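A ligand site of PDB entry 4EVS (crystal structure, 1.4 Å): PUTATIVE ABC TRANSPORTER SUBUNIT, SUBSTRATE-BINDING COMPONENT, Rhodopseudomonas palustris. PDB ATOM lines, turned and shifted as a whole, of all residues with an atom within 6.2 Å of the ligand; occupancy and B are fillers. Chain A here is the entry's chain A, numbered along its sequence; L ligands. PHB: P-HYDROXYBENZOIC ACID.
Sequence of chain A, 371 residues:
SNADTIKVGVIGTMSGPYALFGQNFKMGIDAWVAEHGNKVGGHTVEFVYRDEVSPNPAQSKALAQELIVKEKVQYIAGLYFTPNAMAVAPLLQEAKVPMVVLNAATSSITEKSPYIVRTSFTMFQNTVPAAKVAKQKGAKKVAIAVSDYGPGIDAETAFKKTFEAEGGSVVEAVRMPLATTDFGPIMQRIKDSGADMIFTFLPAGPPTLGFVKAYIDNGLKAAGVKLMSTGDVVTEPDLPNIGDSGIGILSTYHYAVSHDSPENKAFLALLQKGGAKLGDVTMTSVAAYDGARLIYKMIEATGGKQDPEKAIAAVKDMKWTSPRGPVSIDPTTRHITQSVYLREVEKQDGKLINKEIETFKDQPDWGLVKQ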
ATOM      1  N   TYR A  80      18.695 -12.484 -22.460  1.00  0.00           N
ATOM      2  CA  TYR A  80      18.601 -13.901 -22.186  1.00  0.00           C
ATOM      3  C   TYR A  80      19.734 -14.301 -21.236  1.00  0.00           C
ATOM      4  O   TYR A  80      19.494 -14.977 -20.246  1.00  0.00           O
ATOM      5  CB  TYR A  80      18.652 -14.710 -23.457  1.00  0.00           C
ATOM      6  CG  TYR A  80      18.356 -16.193 -23.233  1.00  0.00           C
ATOM      7  CD1 TYR A  80      17.134 -16.592 -22.712  1.00  0.00           C
ATOM      8  CD2 TYR A  80      19.278 -17.165 -23.541  1.00  0.00           C
ATOM      9  CE1 TYR A  80      16.824 -17.904 -22.542  1.00  0.00           C
ATOM     10  CE2 TYR A  80      18.989 -18.508 -23.323  1.00  0.00           C
ATOM     11  CZ  TYR A  80      17.761 -18.870 -22.809  1.00  0.00           C
ATOM     12  OH  TYR A  80      17.431 -20.208 -22.563  1.00  0.00           O
ATOM     13  N   PHE A  81      20.957 -13.857 -21.522  1.00  0.00           N
ATOM     14  CA  PHE A  81      22.151 -14.316 -20.795  1.00  0.00           C
ATOM     15  C   PHE A  81      22.665 -13.328 -19.754  1.00  0.00           C
ATOM     16  O   PHE A  81      22.772 -12.097 -20.017  1.00  0.00           O
ATOM     17  CB  PHE A  81      23.278 -14.583 -21.793  1.00  0.00           C
ATOM     18  CG  PHE A  81      23.046 -15.804 -22.666  1.00  0.00           C
ATOM     19  CD1 PHE A  81      23.120 -17.085 -22.124  1.00  0.00           C
ATOM     20  CD2 PHE A  81      22.795 -15.676 -24.048  1.00  0.00           C
ATOM     21  CE1 PHE A  81      22.891 -18.207 -22.935  1.00  0.00           C
ATOM     22  CE2 PHE A  81      22.567 -16.784 -24.818  1.00  0.00           C
ATOM     23  CZ  PHE A  81      22.679 -18.043 -24.261  1.00  0.00           C
ATOM     24  N   THR A  82      23.033 -13.859 -18.592  1.00  0.00           N
ATOM     25  CA  THR A  82      23.584 -13.049 -17.515  1.00  0.00           C
ATOM     26  C   THR A  82      24.713 -12.095 -17.940  1.00  0.00           C
ATOM     27  O   THR A  82      24.640 -10.919 -17.632  1.00  0.00           O
ATOM     28  CB  THR A  82      24.023 -13.933 -16.353  1.00  0.00           C
ATOM     29  OG1 THR A  82      22.866 -14.343 -15.627  1.00  0.00           O
ATOM     30  CG2 THR A  82      24.945 -13.179 -15.422  1.00  0.00           C
ATOM     31  N   PRO A  83      25.715 -12.576 -18.665  1.00  0.00           N
ATOM     32  CA  PRO A  83      26.815 -11.638 -18.984  1.00  0.00           C
ATOM     33  C   PRO A  83      26.405 -10.475 -19.889  1.00  0.00           C
ATOM     34  O   PRO A  83      27.007  -9.402 -19.855  1.00  0.00           O
ATOM     35  CB  PRO A  83      27.864 -12.545 -19.645  1.00  0.00           C
ATOM     36  CG  PRO A  83      27.175 -13.814 -19.943  1.00  0.00           C
ATOM     37  CD  PRO A  83      26.073 -13.973 -18.942  1.00  0.00           C
ATOM     38  N   ASN A 103      14.898 -12.540 -18.648  1.00  0.00           N
ATOM     39  CA  ASN A 103      15.428 -13.869 -18.367  1.00  0.00           C
ATOM     40  C   ASN A 103      16.618 -13.878 -17.412  1.00  0.00           C
ATOM     41  O   ASN A 103      16.525 -14.443 -16.329  1.00  0.00           O
ATOM     42  CB  ASN A 103      15.755 -14.648 -19.622  1.00  0.00           C
ATOM     43  CG  ASN A 103      16.012 -16.114 -19.283  1.00  0.00           C
ATOM     44  OD1 ASN A 103      15.055 -16.862 -19.017  1.00  0.00           O
ATOM     45  ND2 ASN A 103      17.275 -16.521 -19.259  1.00  0.00           N
ATOM     46  N   ALA A 104      17.729 -13.269 -17.821  1.00  0.00           N
ATOM     47  CA  ALA A 104      19.016 -13.337 -17.124  1.00  0.00           C
ATOM     48  C   ALA A 104      18.789 -13.413 -15.598  1.00  0.00           C
ATOM     49  O   ALA A 104      18.228 -12.501 -15.019  1.00  0.00           O
ATOM     50  CB  ALA A 104      19.876 -12.145 -17.454  1.00  0.00           C
ATOM     51  N   ALA A 105      19.259 -14.510 -14.993  1.00  0.00           N
ATOM     52  CA  ALA A 105      18.784 -14.987 -13.698  1.00  0.00           C
ATOM     53  C   ALA A 105      19.791 -14.925 -12.556  1.00  0.00           C
ATOM     54  O   ALA A 105      19.485 -15.371 -11.463  1.00  0.00           O
ATOM     55  CB  ALA A 105      18.245 -16.412 -13.887  1.00  0.00           C
ATOM     56  N   THR A 106      20.981 -14.343 -12.770  1.00  0.00           N
ATOM     57  CA  THR A 106      21.951 -14.211 -11.675  1.00  0.00           C
ATOM     58  C   THR A 106      21.485 -13.182 -10.671  1.00  0.00           C
ATOM     59  O   THR A 106      21.074 -12.076 -11.050  1.00  0.00           O
ATOM     60  CB  THR A 106      23.378 -13.940 -12.269  1.00  0.00           C
ATOM     61  OG1 THR A 106      23.704 -15.032 -13.103  1.00  0.00           O
ATOM     62  CG2 THR A 106      24.444 -13.775 -11.170  1.00  0.00           C
ATOM     63  N   ILE A 109      22.460  -9.258 -10.551  1.00  0.00           N
ATOM     64  CA  ILE A 109      22.180  -8.340 -11.669  1.00  0.00           C
ATOM     65  C   ILE A 109      21.425  -7.082 -11.235  1.00  0.00           C
ATOM     66  O   ILE A 109      21.736  -5.968 -11.678  1.00  0.00           O
ATOM     67  CB  ILE A 109      21.411  -9.031 -12.821  1.00  0.00           C
ATOM     68  CG1 ILE A 109      22.285 -10.118 -13.475  1.00  0.00           C
ATOM     69  CG2 ILE A 109      20.907  -8.024 -13.877  1.00  0.00           C
ATOM     70  CD1 ILE A 109      21.581 -10.967 -14.575  1.00  0.00           C
ATOM     71  N   PHE A 121      13.166 -14.645 -13.037  1.00  0.00           N
ATOM     72  CA  PHE A 121      13.445 -15.533 -11.919  1.00  0.00           C
ATOM     73  C   PHE A 121      14.908 -15.378 -11.561  1.00  0.00           C
ATOM     74  O   PHE A 121      15.662 -14.759 -12.334  1.00  0.00           O
ATOM     75  CB  PHE A 121      13.165 -16.990 -12.273  1.00  0.00           C
ATOM     76  CG  PHE A 121      13.931 -17.483 -13.482  1.00  0.00           C
ATOM     77  CD1 PHE A 121      13.441 -17.236 -14.750  1.00  0.00           C
ATOM     78  CD2 PHE A 121      15.089 -18.250 -13.349  1.00  0.00           C
ATOM     79  CE1 PHE A 121      14.115 -17.631 -15.876  1.00  0.00           C
ATOM     80  CE2 PHE A 121      15.781 -18.684 -14.461  1.00  0.00           C
ATOM     81  CZ  PHE A 121      15.274 -18.398 -15.742  1.00  0.00           C
ATOM     82  N   MET A 123      18.305 -17.865 -10.029  1.00  0.00           N
ATOM     83  CA  MET A 123      18.740 -19.200  -9.804  1.00  0.00           C
ATOM     84  C   MET A 123      18.541 -19.638  -8.349  1.00  0.00           C
ATOM     85  O   MET A 123      18.073 -20.736  -8.066  1.00  0.00           O
ATOM     86  CB  MET A 123      20.202 -19.357 -10.224  1.00  0.00           C
ATOM     87  CG  MET A 123      20.427 -19.092 -11.691  1.00  0.00           C
ATOM     88  SD  MET A 123      19.273 -20.060 -12.941  1.00  0.00           S
ATOM     89  CE  MET A 123      19.599 -21.829 -12.317  1.00  0.00           C
ATOM     90  N   TYR A 149      29.424 -20.340 -15.414  1.00  0.00           N
ATOM     91  CA  TYR A 149      29.246 -18.889 -15.471  1.00  0.00           C
ATOM     92  C   TYR A 149      28.192 -18.480 -14.411  1.00  0.00           C
ATOM     93  O   TYR A 149      27.702 -19.326 -13.675  1.00  0.00           O
ATOM     94  CB  TYR A 149      28.934 -18.396 -16.892  1.00  0.00           C
ATOM     95  CG  TYR A 149      27.526 -18.537 -17.404  1.00  0.00           C
ATOM     96  CD1 TYR A 149      26.901 -19.765 -17.435  1.00  0.00           C
ATOM     97  CD2 TYR A 149      26.851 -17.450 -17.946  1.00  0.00           C
ATOM     98  CE1 TYR A 149      25.603 -19.909 -17.893  1.00  0.00           C
ATOM     99  CE2 TYR A 149      25.527 -17.580 -18.450  1.00  0.00           C
ATOM    100  CZ  TYR A 149      24.924 -18.825 -18.405  1.00  0.00           C
ATOM    101  OH  TYR A 149      23.639 -18.964 -18.837  1.00  0.00           O
ATOM    102  N   PRO A 151      25.034 -17.835 -13.558  1.00  0.00           N
ATOM    103  CA  PRO A 151      23.841 -18.468 -12.991  1.00  0.00           C
ATOM    104  C   PRO A 151      24.123 -19.913 -12.528  1.00  0.00           C
ATOM    105  O   PRO A 151      23.488 -20.405 -11.600  1.00  0.00           O
ATOM    106  CB  PRO A 151      22.815 -18.377 -14.127  1.00  0.00           C
ATOM    107  CG  PRO A 151      23.670 -18.266 -15.387  1.00  0.00           C
ATOM    108  CD  PRO A 151      24.849 -17.458 -14.968  1.00  0.00           C
ATOM    109  N   PHE A 201      22.097 -27.401 -13.739  1.00  0.00           N
ATOM    110  CA  PHE A 201      21.638 -26.241 -14.499  1.00  0.00           C
ATOM    111  C   PHE A 201      22.589 -26.038 -15.685  1.00  0.00           C
ATOM    112  O   PHE A 201      23.820 -26.035 -15.497  1.00  0.00           O
ATOM    113  CB  PHE A 201      21.612 -24.932 -13.694  1.00  0.00           C
ATOM    114  CG  PHE A 201      21.594 -23.700 -14.581  1.00  0.00           C
ATOM    115  CD1 PHE A 201      20.398 -23.278 -15.162  1.00  0.00           C
ATOM    116  CD2 PHE A 201      22.751 -23.021 -14.936  1.00  0.00           C
ATOM    117  CE1 PHE A 201      20.364 -22.230 -16.019  1.00  0.00           C
ATOM    118  CE2 PHE A 201      22.692 -21.930 -15.768  1.00  0.00           C
ATOM    119  CZ  PHE A 201      21.512 -21.556 -16.314  1.00  0.00           C
ATOM    120  N   LEU A 202      22.022 -25.833 -16.874  1.00  0.00           N
ATOM    121  CA  LEU A 202      22.678 -25.240 -18.060  1.00  0.00           C
ATOM    122  C   LEU A 202      21.631 -24.288 -18.663  1.00  0.00           C
ATOM    123  O   LEU A 202      20.422 -24.450 -18.433  1.00  0.00           O
ATOM    124  CB  LEU A 202      23.088 -26.306 -19.095  1.00  0.00           C
ATOM    125  CG  LEU A 202      23.803 -27.551 -18.576  1.00  0.00           C
ATOM    126  CD1 LEU A 202      22.809 -28.611 -18.135  1.00  0.00           C
ATOM    127  CD2 LEU A 202      24.764 -28.090 -19.659  1.00  0.00           C
ATOM    128  N   PRO A 203      22.073 -23.292 -19.440  1.00  0.00           N
ATOM    129  CA  PRO A 203      21.073 -22.405 -20.056  1.00  0.00           C
ATOM    130  C   PRO A 203      20.179 -23.191 -21.033  1.00  0.00           C
ATOM    131  O   PRO A 203      20.686 -24.051 -21.784  1.00  0.00           O
ATOM    132  CB  PRO A 203      21.927 -21.364 -20.760  1.00  0.00           C
ATOM    133  CG  PRO A 203      23.233 -21.998 -20.958  1.00  0.00           C
ATOM    134  CD  PRO A 203      23.435 -22.909 -19.833  1.00  0.00           C
ATOM    135  N   ALA A 204      18.871 -22.929 -20.973  1.00  0.00           N
ATOM    136  CA  ALA A 204      17.916 -23.645 -21.820  1.00  0.00           C
ATOM    137  C   ALA A 204      18.294 -23.455 -23.283  1.00  0.00           C
ATOM    138  O   ALA A 204      18.571 -22.346 -23.741  1.00  0.00           O
ATOM    139  CB  ALA A 204      16.484 -23.148 -21.604  1.00  0.00           C
ATOM    140  N   ASP A 232      14.830 -24.672 -16.401  1.00  0.00           N
ATOM    141  CA  ASP A 232      15.695 -24.406 -17.553  1.00  0.00           C
ATOM    142  C   ASP A 232      16.047 -25.650 -18.350  1.00  0.00           C
ATOM    143  O   ASP A 232      16.274 -25.575 -19.582  1.00  0.00           O
ATOM    144  CB  ASP A 232      16.982 -23.717 -17.055  1.00  0.00           C
ATOM    145  CG  ASP A 232      16.676 -22.534 -16.205  1.00  0.00           C
ATOM    146  OD1 ASP A 232      16.399 -21.458 -16.763  1.00  0.00           O
ATOM    147  OD2 ASP A 232      16.616 -22.715 -14.962  1.00  0.00           O
ATOM    148  N   THR A 235      12.558 -27.267 -20.691  1.00  0.00           N
ATOM    149  CA  THR A 235      11.602 -26.347 -21.287  1.00  0.00           C
ATOM    150  C   THR A 235      10.659 -27.093 -22.257  1.00  0.00           C
ATOM    151  O   THR A 235      11.050 -28.064 -22.942  1.00  0.00           O
ATOM    152  CB  THR A 235      12.265 -25.149 -21.958  1.00  0.00           C
ATOM    153  OG1 THR A 235      13.096 -25.581 -23.029  1.00  0.00           O
ATOM    154  CG2 THR A 235      13.009 -24.257 -20.959  1.00  0.00           C
ATOM    155  N   TYR A 253      10.535 -24.662 -10.893  1.00  0.00           N
ATOM    156  CA  TYR A 253      10.451 -23.489 -11.738  1.00  0.00           C
ATOM    157  C   TYR A 253       9.200 -22.722 -11.418  1.00  0.00           C
ATOM    158  O   TYR A 253       8.208 -23.262 -10.924  1.00  0.00           O
ATOM    159  CB  TYR A 253      10.372 -23.869 -13.218  1.00  0.00           C
ATOM    160  CG  TYR A 253      11.232 -23.099 -14.208  1.00  0.00           C
ATOM    161  CD1 TYR A 253      10.786 -22.924 -15.524  1.00  0.00           C
ATOM    162  CD2 TYR A 253      12.471 -22.607 -13.881  1.00  0.00           C
ATOM    163  CE1 TYR A 253      11.608 -22.385 -16.470  1.00  0.00           C
ATOM    164  CE2 TYR A 253      13.275 -21.999 -14.827  1.00  0.00           C
ATOM    165  CZ  TYR A 253      12.854 -21.892 -16.102  1.00  0.00           C
ATOM    166  OH  TYR A 253      13.650 -21.325 -17.066  1.00  0.00           O
ATOM    167  N   MET A 283       9.088 -20.310 -20.934  1.00  0.00           N
ATOM    168  CA  MET A 283       9.103 -19.355 -19.815  1.00  0.00           C
ATOM    169  C   MET A 283       9.392 -17.922 -20.186  1.00  0.00           C
ATOM    170  O   MET A 283       8.892 -16.995 -19.539  1.00  0.00           O
ATOM    171  CB  MET A 283      10.039 -19.825 -18.714  1.00  0.00           C
ATOM    172  CG  MET A 283      11.509 -19.549 -18.943  1.00  0.00           C
ATOM    173  SD  MET A 283      12.297 -20.464 -20.514  1.00  0.00           S
ATOM    174  CE  MET A 283      14.174 -20.049 -20.119  1.00  0.00           C
HETATM  175  C1' PHB L   1      21.369 -16.717 -17.695  1.00  0.00           C
HETATM  176  O1' PHB L   1      22.394 -16.592 -18.417  1.00  0.00           O
HETATM  177  O2' PHB L   1      21.166 -16.010 -16.652  1.00  0.00           O
HETATM  178  C1  PHB L   1      20.403 -17.791 -18.040  1.00  0.00           C
HETATM  179  C2  PHB L   1      20.282 -18.249 -19.331  1.00  0.00           C
HETATM  180  C3  PHB L   1      19.409 -19.287 -19.621  1.00  0.00           C
HETATM  181  C4  PHB L   1      18.576 -19.832 -18.629  1.00  0.00           C
HETATM  182  C5  PHB L   1      18.655 -19.323 -17.340  1.00  0.00           C
HETATM  183  C6  PHB L   1      19.576 -18.326 -17.057  1.00  0.00           C
HETATM  184  O4  PHB L   1      17.718 -20.840 -18.959  1.00  0.00           O
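The side-chain hydroxyl of Thr 82 is in hydrogen-bond range of an oxygen (O2') of the ligand, 2.6 Å away.
O1' of the ligand sits at hydrogen-bond distance from N of Thr 82 (2.8 Å).
The backbone NH of Ala 105 is in hydrogen-bond range of an oxygen (O2') of the ligand (2.9 Å).
OH of Tyr 149 sits at hydrogen-bond distance from O1' of the ligand (2.7 Å).
The backbone NH (N) of Ala 204 is in hydrogen-bond range of an oxygen (O4) of the ligand.
An oxygen (O4) of the ligand lies within hydrogen-bond range of the side-chain carboxylate (OD1) of Asp 232 (2.6 Å).
O of Ala 204 sits at hydrogen-bond distance from OH of Tyr 80.
The side-chain carboxylate (OD1) of Asp 232 lies within hydrogen-bond range of the side-chain hydroxyl (OH) of Tyr 253 (2.8 Å).
OG1 of Thr 82 sits at hydrogen-bond distance from OG1 of Thr 106, at 2.7 Å.
The side-chain amide nitrogen (ND2) of Asn 103 lies within hydrogen-bond range of the backbone carbonyl oxygen (O) of Tyr 80, 2.9 Å away.
The backbone NH (N) of Ala 104 sits at hydrogen-bond distance from the backbone carbonyl oxygen (O) of Tyr 80, at 3.5 Å.
O of Ala 105 is in hydrogen-bond range of N of Met 123, at 3.1 Å.
Tyr 80 touches the ligand.
CA of Phe 81 touches O1' of the ligand (3.3 Å).
ND2 of Asn 103 touches C2 of the ligand, 3.5 Å away.
CA of Ala 104 touches O2' of the ligand, at 3.5 Å.
Phe 121 touches the ligand (CZ to C5, 3.9 Å).
Pro 151 touches the ligand (CG to O2', 3.6 Å).
CE1 of Phe 201 touches C5 of the ligand, at 3.6 Å.
Pro 203 touches the ligand (CB to C3, 3.5 Å).
CE of Met 283 touches O4 of the ligand, 3.8 Å away.
Hydrophobic or aromatic side chains within 4 Å of the ligand: Tyr 80, Phe 81, Ala 105, Phe 121, Tyr 149, Pro 151, Phe 201, Pro 203, Ala 204 and Met 283.
Of the 21 residues printed, 14 come within 4 Å of the ligand.
The nearest printed residue that does not touch the ligand is Thr 106 (4.2 Å).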
